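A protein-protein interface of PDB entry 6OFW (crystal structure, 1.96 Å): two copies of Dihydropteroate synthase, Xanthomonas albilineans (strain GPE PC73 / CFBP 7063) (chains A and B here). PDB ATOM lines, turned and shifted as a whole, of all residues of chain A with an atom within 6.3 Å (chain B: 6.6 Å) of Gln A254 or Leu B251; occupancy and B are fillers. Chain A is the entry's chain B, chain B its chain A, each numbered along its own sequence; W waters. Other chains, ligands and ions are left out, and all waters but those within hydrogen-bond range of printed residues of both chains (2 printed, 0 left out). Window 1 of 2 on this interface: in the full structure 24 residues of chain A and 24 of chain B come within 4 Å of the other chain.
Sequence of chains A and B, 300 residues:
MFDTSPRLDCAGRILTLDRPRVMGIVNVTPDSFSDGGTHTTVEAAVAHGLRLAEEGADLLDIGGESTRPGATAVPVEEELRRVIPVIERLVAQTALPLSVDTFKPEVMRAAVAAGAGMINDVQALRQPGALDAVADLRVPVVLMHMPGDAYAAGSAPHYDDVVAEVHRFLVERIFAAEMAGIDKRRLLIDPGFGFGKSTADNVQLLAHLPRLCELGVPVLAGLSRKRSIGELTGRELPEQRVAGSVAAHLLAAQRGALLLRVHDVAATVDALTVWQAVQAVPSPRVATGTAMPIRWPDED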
ATOM      1  N   PRO A  20     -28.271   3.444  22.195  1.00  0.00           N
ATOM      2  CA  PRO A  20     -27.171   2.905  21.370  1.00  0.00           C
ATOM      3  C   PRO A  20     -27.151   1.380  21.377  1.00  0.00           C
ATOM      4  O   PRO A  20     -27.290   0.741  22.415  1.00  0.00           O
ATOM      5  CB  PRO A  20     -25.918   3.519  22.000  1.00  0.00           C
ATOM      6  CG  PRO A  20     -26.434   4.778  22.677  1.00  0.00           C
ATOM      7  CD  PRO A  20     -27.756   4.344  23.244  1.00  0.00           C
ATOM      8  N   PRO A 210     -21.294  14.883  17.144  1.00  0.00           N
ATOM      9  CA  PRO A 210     -22.650  15.472  17.127  1.00  0.00           C
ATOM     10  C   PRO A 210     -23.003  16.212  15.838  1.00  0.00           C
ATOM     11  O   PRO A 210     -24.173  16.243  15.497  1.00  0.00           O
ATOM     12  CB  PRO A 210     -22.633  16.420  18.332  1.00  0.00           C
ATOM     13  CG  PRO A 210     -21.658  15.814  19.255  1.00  0.00           C
ATOM     14  CD  PRO A 210     -20.563  15.344  18.346  1.00  0.00           C
ATOM     15  N   ALA A 247     -13.945   2.419  25.849  1.00  0.00           N
ATOM     16  CA  ALA A 247     -14.025   3.851  26.157  1.00  0.00           C
ATOM     17  C   ALA A 247     -14.396   4.674  24.926  1.00  0.00           C
ATOM     18  O   ALA A 247     -15.264   5.539  25.021  1.00  0.00           O
ATOM     19  CB  ALA A 247     -12.709   4.344  26.722  1.00  0.00           C
ATOM     20  N   HIS A 249     -16.003   3.725  22.226  1.00  0.00           N
ATOM     21  CA  HIS A 249     -17.396   3.436  21.886  1.00  0.00           C
ATOM     22  C   HIS A 249     -18.387   4.084  22.845  1.00  0.00           C
ATOM     23  O   HIS A 249     -19.425   4.575  22.383  1.00  0.00           O
ATOM     24  CB  HIS A 249     -17.639   1.943  21.720  1.00  0.00           C
ATOM     25  CG  HIS A 249     -16.948   1.412  20.496  1.00  0.00           C
ATOM     26  ND1 HIS A 249     -16.003   0.413  20.575  1.00  0.00           N
ATOM     27  CD2 HIS A 249     -17.068   1.797  19.210  1.00  0.00           C
ATOM     28  CE1 HIS A 249     -15.582   0.216  19.345  1.00  0.00           C
ATOM     29  NE2 HIS A 249     -16.192   1.027  18.487  1.00  0.00           N
ATOM     30  N   LEU A 250     -18.051   4.168  24.152  1.00  0.00           N
ATOM     31  CA  LEU A 250     -18.906   4.863  25.110  1.00  0.00           C
ATOM     32  C   LEU A 250     -18.951   6.335  24.774  1.00  0.00           C
ATOM     33  O   LEU A 250     -20.036   6.917  24.770  1.00  0.00           O
ATOM     34  CB  LEU A 250     -18.396   4.646  26.555  1.00  0.00           C
ATOM     35  CG  LEU A 250     -19.192   5.332  27.672  1.00  0.00           C
ATOM     36  CD1 LEU A 250     -20.685   4.945  27.605  1.00  0.00           C
ATOM     37  CD2 LEU A 250     -18.573   5.031  29.048  1.00  0.00           C
ATOM     38  N   LEU A 251     -17.786   6.950  24.450  1.00  0.00           N
ATOM     39  CA  LEU A 251     -17.715   8.360  24.052  1.00  0.00           C
ATOM     40  C   LEU A 251     -18.501   8.608  22.761  1.00  0.00           C
ATOM     41  O   LEU A 251     -19.171   9.641  22.640  1.00  0.00           O
ATOM     42  CB  LEU A 251     -16.238   8.826  23.879  1.00  0.00           C
ATOM     43  CG  LEU A 251     -15.360   8.791  25.142  1.00  0.00           C
ATOM     44  CD1 LEU A 251     -13.914   9.036  24.809  1.00  0.00           C
ATOM     45  CD2 LEU A 251     -15.825   9.809  26.173  1.00  0.00           C
ATOM     46  N   ALA A 252     -18.415   7.669  21.798  1.00  0.00           N
ATOM     47  CA  ALA A 252     -19.149   7.763  20.522  1.00  0.00           C
ATOM     48  C   ALA A 252     -20.656   7.756  20.820  1.00  0.00           C
ATOM     49  O   ALA A 252     -21.367   8.643  20.327  1.00  0.00           O
ATOM     50  CB  ALA A 252     -18.772   6.593  19.598  1.00  0.00           C
ATOM     51  N   ALA A 253     -21.123   6.844  21.706  1.00  0.00           N
ATOM     52  CA  ALA A 253     -22.533   6.819  22.129  1.00  0.00           C
ATOM     53  C   ALA A 253     -22.945   8.125  22.848  1.00  0.00           C
ATOM     54  O   ALA A 253     -24.022   8.657  22.580  1.00  0.00           O
ATOM     55  CB  ALA A 253     -22.795   5.632  23.030  1.00  0.00           C
ATOM     56  N   GLN A 254     -22.077   8.669  23.720  1.00  0.00           N
ATOM     57  CA  GLN A 254     -22.378   9.932  24.415  1.00  0.00           C
ATOM     58  C   GLN A 254     -22.516  11.082  23.430  1.00  0.00           C
ATOM     59  O   GLN A 254     -23.251  12.035  23.695  1.00  0.00           O
ATOM     60  CB  GLN A 254     -21.286  10.271  25.439  1.00  0.00           C
ATOM     61  CG  GLN A 254     -21.342   9.366  26.661  1.00  0.00           C
ATOM     62  CD  GLN A 254     -20.190   9.533  27.619  1.00  0.00           C
ATOM     63  OE1 GLN A 254     -19.074   9.926  27.255  1.00  0.00           O
ATOM     64  NE2 GLN A 254     -20.440   9.214  28.871  1.00  0.00           N
ATOM     65  N   ARG A 255     -21.776  10.997  22.304  1.00  0.00           N
ATOM     66  CA  ARG A 255     -21.727  12.027  21.282  1.00  0.00           C
ATOM     67  C   ARG A 255     -22.709  11.785  20.128  1.00  0.00           C
ATOM     68  O   ARG A 255     -22.594  12.425  19.088  1.00  0.00           O
ATOM     69  CB  ARG A 255     -20.279  12.246  20.806  1.00  0.00           C
ATOM     70  CG  ARG A 255     -19.505  13.101  21.819  1.00  0.00           C
ATOM     71  CD  ARG A 255     -18.008  12.862  21.849  1.00  0.00           C
ATOM     72  NE  ARG A 255     -17.352  13.672  22.883  1.00  0.00           N
ATOM     73  CZ  ARG A 255     -17.340  13.416  24.191  1.00  0.00           C
ATOM     74  NH1 ARG A 255     -17.995  12.366  24.678  1.00  0.00           N
ATOM     75  NH2 ARG A 255     -16.709  14.230  25.026  1.00  0.00           N
ATOM     76  N   GLY A 256     -23.690  10.920  20.343  1.00  0.00           N
ATOM     77  CA  GLY A 256     -24.747  10.706  19.364  1.00  0.00           C
ATOM     78  C   GLY A 256     -24.819   9.413  18.579  1.00  0.00           C
ATOM     79  O   GLY A 256     -25.863   9.154  17.970  1.00  0.00           O
ATOM     80  N   ALA A 257     -23.746   8.578  18.572  1.00  0.00           N
ATOM     81  CA  ALA A 257     -23.788   7.327  17.810  1.00  0.00           C
ATOM     82  C   ALA A 257     -24.887   6.427  18.341  1.00  0.00           C
ATOM     83  O   ALA A 257     -25.036   6.305  19.562  1.00  0.00           O
ATOM     84  CB  ALA A 257     -22.444   6.614  17.853  1.00  0.00           C
ATOM     85  N   ALA A 271     -20.409  -1.433  29.600  1.00  0.00           N
ATOM     86  CA  ALA A 271     -20.121   0.007  29.645  1.00  0.00           C
ATOM     87  C   ALA A 271     -21.363   0.841  29.359  1.00  0.00           C
ATOM     88  O   ALA A 271     -21.655   1.792  30.089  1.00  0.00           O
ATOM     89  CB  ALA A 271     -19.013   0.368  28.648  1.00  0.00           C
ATOM     90  N   VAL A 274     -24.010   0.695  32.308  1.00  0.00           N
ATOM     91  CA  VAL A 274     -23.656   1.590  33.407  1.00  0.00           C
ATOM     92  C   VAL A 274     -24.023   3.025  33.024  1.00  0.00           C
ATOM     93  O   VAL A 274     -24.670   3.719  33.811  1.00  0.00           O
ATOM     94  CB  VAL A 274     -22.168   1.453  33.861  1.00  0.00           C
ATOM     95  CG1 VAL A 274     -21.813   2.503  34.929  1.00  0.00           C
ATOM     96  CG2 VAL A 274     -21.877   0.034  34.367  1.00  0.00           C
ATOM     97  N   TRP A 275     -23.629   3.463  31.813  1.00  0.00           N
ATOM     98  CA  TRP A 275     -23.941   4.807  31.343  1.00  0.00           C
ATOM     99  C   TRP A 275     -25.438   5.066  31.248  1.00  0.00           C
ATOM    100  O   TRP A 275     -25.874   6.141  31.648  1.00  0.00           O
ATOM    101  CB  TRP A 275     -23.258   5.111  30.015  1.00  0.00           C
ATOM    102  CG  TRP A 275     -23.729   6.373  29.352  1.00  0.00           C
ATOM    103  CD1 TRP A 275     -23.620   7.646  29.826  1.00  0.00           C
ATOM    104  CD2 TRP A 275     -24.304   6.477  28.047  1.00  0.00           C
ATOM    105  NE1 TRP A 275     -24.129   8.535  28.904  1.00  0.00           N
ATOM    106  CE2 TRP A 275     -24.557   7.843  27.806  1.00  0.00           C
ATOM    107  CE3 TRP A 275     -24.651   5.540  27.063  1.00  0.00           C
ATOM    108  CZ2 TRP A 275     -25.122   8.301  26.608  1.00  0.00           C
ATOM    109  CZ3 TRP A 275     -25.258   5.990  25.897  1.00  0.00           C
ATOM    110  CH2 TRP A 275     -25.473   7.357  25.673  1.00  0.00           C
ATOM    111  N   GLN A 276     -26.215   4.089  30.736  1.00  0.00           N
ATOM    112  CA  GLN A 276     -27.675   4.221  30.632  1.00  0.00           C
ATOM    113  C   GLN A 276     -28.281   4.453  32.022  1.00  0.00           C
ATOM    114  O   GLN A 276     -29.132   5.327  32.152  1.00  0.00           O
ATOM    115  CB  GLN A 276     -28.312   2.980  29.956  1.00  0.00           C
ATOM    116  CG  GLN A 276     -28.214   2.990  28.424  1.00  0.00           C
ATOM    117  CD  GLN A 276     -28.962   4.124  27.749  1.00  0.00           C
ATOM    118  OE1 GLN A 276     -30.105   4.462  28.091  1.00  0.00           O
ATOM    119  NE2 GLN A 276     -28.333   4.728  26.757  1.00  0.00           N
ATOM    120  N   VAL A 278     -26.867   5.835  34.713  1.00  0.00           N
ATOM    121  CA  VAL A 278     -26.501   7.184  35.138  1.00  0.00           C
ATOM    122  C   VAL A 278     -27.330   8.223  34.372  1.00  0.00           C
ATOM    123  O   VAL A 278     -27.866   9.148  34.989  1.00  0.00           O
ATOM    124  CB  VAL A 278     -24.972   7.399  34.991  1.00  0.00           C
ATOM    125  CG1 VAL A 278     -24.570   8.854  35.195  1.00  0.00           C
ATOM    126  CG2 VAL A 278     -24.210   6.486  35.934  1.00  0.00           C
ATOM    127  N   LEU B 206     -23.411   9.002  41.710  1.00  0.00           N
ATOM    128  CA  LEU B 206     -22.561   9.100  40.514  1.00  0.00           C
ATOM    129  C   LEU B 206     -23.131  10.124  39.536  1.00  0.00           C
ATOM    130  O   LEU B 206     -22.391  10.988  39.054  1.00  0.00           O
ATOM    131  CB  LEU B 206     -22.411   7.721  39.850  1.00  0.00           C
ATOM    132  CG  LEU B 206     -21.550   7.640  38.567  1.00  0.00           C
ATOM    133  CD1 LEU B 206     -20.201   8.309  38.748  1.00  0.00           C
ATOM    134  CD2 LEU B 206     -21.334   6.189  38.146  1.00  0.00           C
ATOM    135  N   LEU B 209     -22.653  13.564  41.013  1.00  0.00           N
ATOM    136  CA  LEU B 209     -21.287  13.846  41.469  1.00  0.00           C
ATOM    137  C   LEU B 209     -20.855  15.310  41.293  1.00  0.00           C
ATOM    138  O   LEU B 209     -20.180  15.793  42.204  1.00  0.00           O
ATOM    139  CB  LEU B 209     -20.262  12.894  40.819  1.00  0.00           C
ATOM    140  CG  LEU B 209     -19.005  12.591  41.624  1.00  0.00           C
ATOM    141  CD1 LEU B 209     -19.346  11.910  42.957  1.00  0.00           C
ATOM    142  CD2 LEU B 209     -18.072  11.674  40.829  1.00  0.00           C
ATOM    143  N   VAL B 246     -14.612   0.057  34.796  1.00  0.00           N
ATOM    144  CA  VAL B 246     -13.815   0.992  33.961  1.00  0.00           C
ATOM    145  C   VAL B 246     -14.772   2.074  33.417  1.00  0.00           C
ATOM    146  O   VAL B 246     -14.461   3.263  33.494  1.00  0.00           O
ATOM    147  CB  VAL B 246     -13.041   0.239  32.831  1.00  0.00           C
ATOM    148  CG1 VAL B 246     -12.399   1.222  31.845  1.00  0.00           C
ATOM    149  CG2 VAL B 246     -11.970  -0.685  33.412  1.00  0.00           C
ATOM    150  N   ALA B 247     -15.982   1.662  32.977  1.00  0.00           N
ATOM    151  CA  ALA B 247     -16.987   2.620  32.496  1.00  0.00           C
ATOM    152  C   ALA B 247     -17.447   3.553  33.624  1.00  0.00           C
ATOM    153  O   ALA B 247     -17.545   4.753  33.397  1.00  0.00           O
ATOM    154  CB  ALA B 247     -18.175   1.869  31.921  1.00  0.00           C
ATOM    155  N   ALA B 248     -17.712   3.017  34.835  1.00  0.00           N
ATOM    156  CA  ALA B 248     -18.143   3.827  36.007  1.00  0.00           C
ATOM    157  C   ALA B 248     -17.097   4.842  36.363  1.00  0.00           C
ATOM    158  O   ALA B 248     -17.436   5.989  36.630  1.00  0.00           O
ATOM    159  CB  ALA B 248     -18.418   2.939  37.216  1.00  0.00           C
ATOM    160  N   HIS B 249     -15.818   4.442  36.333  1.00  0.00           N
ATOM    161  CA  HIS B 249     -14.723   5.361  36.647  1.00  0.00           C
ATOM    162  C   HIS B 249     -14.541   6.436  35.596  1.00  0.00           C
ATOM    163  O   HIS B 249     -14.290   7.578  35.963  1.00  0.00           O
ATOM    164  CB  HIS B 249     -13.437   4.615  36.953  1.00  0.00           C
ATOM    165  CG  HIS B 249     -13.539   3.879  38.256  1.00  0.00           C
ATOM    166  ND1 HIS B 249     -13.376   2.512  38.321  1.00  0.00           N
ATOM    167  CD2 HIS B 249     -13.810   4.350  39.499  1.00  0.00           C
ATOM    168  CE1 HIS B 249     -13.559   2.198  39.586  1.00  0.00           C
ATOM    169  NE2 HIS B 249     -13.839   3.270  40.329  1.00  0.00           N
ATOM    170  N   LEU B 250     -14.732   6.105  34.297  1.00  0.00           N
ATOM    171  CA  LEU B 250     -14.703   7.122  33.252  1.00  0.00           C
ATOM    172  C   LEU B 250     -15.833   8.132  33.467  1.00  0.00           C
ATOM    173  O   LEU B 250     -15.600   9.331  33.385  1.00  0.00           O
ATOM    174  CB  LEU B 250     -14.825   6.468  31.850  1.00  0.00           C
ATOM    175  CG  LEU B 250     -14.797   7.440  30.666  1.00  0.00           C
ATOM    176  CD1 LEU B 250     -13.537   8.354  30.725  1.00  0.00           C
ATOM    177  CD2 LEU B 250     -14.880   6.684  29.322  1.00  0.00           C
ATOM    178  N   LEU B 251     -17.062   7.642  33.764  1.00  0.00           N
ATOM    179  CA  LEU B 251     -18.217   8.524  34.035  1.00  0.00           C
ATOM    180  C   LEU B 251     -17.976   9.387  35.262  1.00  0.00           C
ATOM    181  O   LEU B 251     -18.358  10.568  35.260  1.00  0.00           O
ATOM    182  CB  LEU B 251     -19.527   7.695  34.221  1.00  0.00           C
ATOM    183  CG  LEU B 251     -19.995   6.876  33.006  1.00  0.00           C
ATOM    184  CD1 LEU B 251     -21.128   5.941  33.392  1.00  0.00           C
ATOM    185  CD2 LEU B 251     -20.421   7.742  31.847  1.00  0.00           C
ATOM    186  N   ALA B 252     -17.347   8.808  36.329  1.00  0.00           N
ATOM    187  CA  ALA B 252     -17.014   9.534  37.546  1.00  0.00           C
ATOM    188  C   ALA B 252     -16.036  10.668  37.205  1.00  0.00           C
ATOM    189  O   ALA B 252     -16.294  11.817  37.588  1.00  0.00           O
ATOM    190  CB  ALA B 252     -16.406   8.592  38.590  1.00  0.00           C
ATOM    191  N   ALA B 253     -14.989  10.373  36.396  1.00  0.00           N
ATOM    192  CA  ALA B 253     -14.047  11.420  35.932  1.00  0.00           C
ATOM    193  C   ALA B 253     -14.773  12.501  35.084  1.00  0.00           C
ATOM    194  O   ALA B 253     -14.530  13.691  35.272  1.00  0.00           O
ATOM    195  CB  ALA B 253     -12.927  10.807  35.124  1.00  0.00           C
ATOM    196  N   GLN B 254     -15.697  12.096  34.197  1.00  0.00           N
ATOM    197  CA  GLN B 254     -16.451  13.067  33.380  1.00  0.00           C
ATOM    198  C   GLN B 254     -17.304  13.976  34.251  1.00  0.00           C
ATOM    199  O   GLN B 254     -17.536  15.125  33.889  1.00  0.00           O
ATOM    200  CB  GLN B 254     -17.355  12.360  32.363  1.00  0.00           C
ATOM    201  CG  GLN B 254     -16.561  11.717  31.229  1.00  0.00           C
ATOM    202  CD  GLN B 254     -17.393  10.875  30.296  1.00  0.00           C
ATOM    203  OE1 GLN B 254     -18.398  10.270  30.662  1.00  0.00           O
ATOM    204  NE2 GLN B 254     -16.973  10.813  29.062  1.00  0.00           N
ATOM    205  N   ARG B 255     -17.760  13.455  35.398  1.00  0.00           N
ATOM    206  CA  ARG B 255     -18.633  14.164  36.333  1.00  0.00           C
ATOM    207  C   ARG B 255     -17.860  14.862  37.475  1.00  0.00           C
ATOM    208  O   ARG B 255     -18.459  15.293  38.454  1.00  0.00           O
ATOM    209  CB  ARG B 255     -19.743  13.229  36.840  1.00  0.00           C
ATOM    210  CG  ARG B 255     -20.828  13.099  35.777  1.00  0.00           C
ATOM    211  CD  ARG B 255     -21.630  11.825  35.857  1.00  0.00           C
ATOM    212  NE  ARG B 255     -22.563  11.657  34.731  1.00  0.00           N
ATOM    213  CZ  ARG B 255     -23.704  12.322  34.557  1.00  0.00           C
ATOM    214  NH1 ARG B 255     -24.087  13.242  35.431  1.00  0.00           N
ATOM    215  NH2 ARG B 255     -24.474  12.065  33.507  1.00  0.00           N
ATOM    216  N   GLY B 256     -16.555  15.048  37.297  1.00  0.00           N
ATOM    217  CA  GLY B 256     -15.766  15.814  38.246  1.00  0.00           C
ATOM    218  C   GLY B 256     -14.782  15.113  39.160  1.00  0.00           C
ATOM    219  O   GLY B 256     -13.962  15.808  39.765  1.00  0.00           O
ATOM    220  N   ALA B 257     -14.812  13.755  39.258  1.00  0.00           N
ATOM    221  CA  ALA B 257     -13.860  13.067  40.141  1.00  0.00           C
ATOM    222  C   ALA B 257     -12.435  13.296  39.651  1.00  0.00           C
ATOM    223  O   ALA B 257     -12.188  13.222  38.435  1.00  0.00           O
ATOM    224  CB  ALA B 257     -14.157  11.577  40.197  1.00  0.00           C
ATOM    225  N   TRP B 275     -10.333   9.305  26.555  1.00  0.00           N
ATOM    226  CA  TRP B 275     -11.180  10.441  26.898  1.00  0.00           C
ATOM    227  C   TRP B 275     -10.430  11.758  26.915  1.00  0.00           C
ATOM    228  O   TRP B 275     -10.957  12.745  26.403  1.00  0.00           O
ATOM    229  CB  TRP B 275     -11.912  10.214  28.218  1.00  0.00           C
ATOM    230  CG  TRP B 275     -12.615  11.428  28.755  1.00  0.00           C
ATOM    231  CD1 TRP B 275     -13.642  12.113  28.175  1.00  0.00           C
ATOM    232  CD2 TRP B 275     -12.383  12.052  30.021  1.00  0.00           C
ATOM    233  NE1 TRP B 275     -14.038  13.151  28.987  1.00  0.00           N
ATOM    234  CE2 TRP B 275     -13.286  13.133  30.130  1.00  0.00           C
ATOM    235  CE3 TRP B 275     -11.477  11.816  31.070  1.00  0.00           C
ATOM    236  CZ2 TRP B 275     -13.329  13.963  31.256  1.00  0.00           C
ATOM    237  CZ3 TRP B 275     -11.498  12.665  32.168  1.00  0.00           C
ATOM    238  CH2 TRP B 275     -12.420  13.719  32.253  1.00  0.00           C
HETATM  239  O   HOH W   1     -27.307  11.870  34.684  1.00  0.00           O
HETATM  240  O   HOH W   2     -16.720  14.958  28.359  1.00  0.00           O
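Printed residues of chain B that touch a printed residue of chain A: Leu B206, Ala B247, Leu B251, Gln B254, Arg B255 and Trp B275. Hydrophobic or aromatic side chains of chain B within 4 Å of the printed part of chain A: Leu B206, Ala B247, Leu B251 and Trp B275. Printed residues of chain A that touch a printed residue of chain B: Leu A251, Gln A254, Ala A271, Val A274, Trp A275 and Val A278. Among the printed residues, no Asp or Glu carboxylate lies within 4 Å of a Lys or Arg side-chain nitrogen of the other chain.
Gln A254 touches just these residues of chain B: Leu B251 and Gln B254. Of chain A, only Gln A254 (3.3 Å), Val A274 (3.8 Å) and Trp A275 (3.7 Å) come within 4 Å of Leu B251. Printed residues of chain A within 4 Å of Arg B255: Val A278 (3.5 Å). Of the printed residues of chain A, Gln B254 touches Leu A251 (3.3 Å) and Gln A254 (2.9 Å). Printed residues of chain A within 4 Å of Leu B206: Val A278.
Leu A251 touches Gln B254, and with the chains exchanged Gln A254 touches Leu B251. Leu A251 touches Trp B275, and with the chains exchanged Trp A275 touches Leu B251. Gln B254 touches its own counterpart, Gln A254.
Water W1 bridges O of Val A278 (2.8 Å) and NH2 of Arg B255 (3.1 Å). Water W2 lies within hydrogen-bond range of NE1 of Trp B275 and NH2 of Arg A255.
The side-chain amide oxygen (OE1) of Gln A254 lies within hydrogen-bond range of the side-chain amide nitrogen (NE2) of Gln B254 (2.9 Å).
Among the printed residues, pairs that only touch across the chains: Leu A251 with Gln B254 (3.3 Å), Leu A251 with Trp B275 (3.7 Å), Gln A254 with Leu B251 (3.3 Å), Ala A271 with Ala B247 (3.5 Å), Val A274 with Leu B251 (3.8 Å), Trp A275 with Leu B251 (3.7 Å), Val A278 with Leu B206 (3.6 Å) and Val A278 with Arg B255 (3.5 Å).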
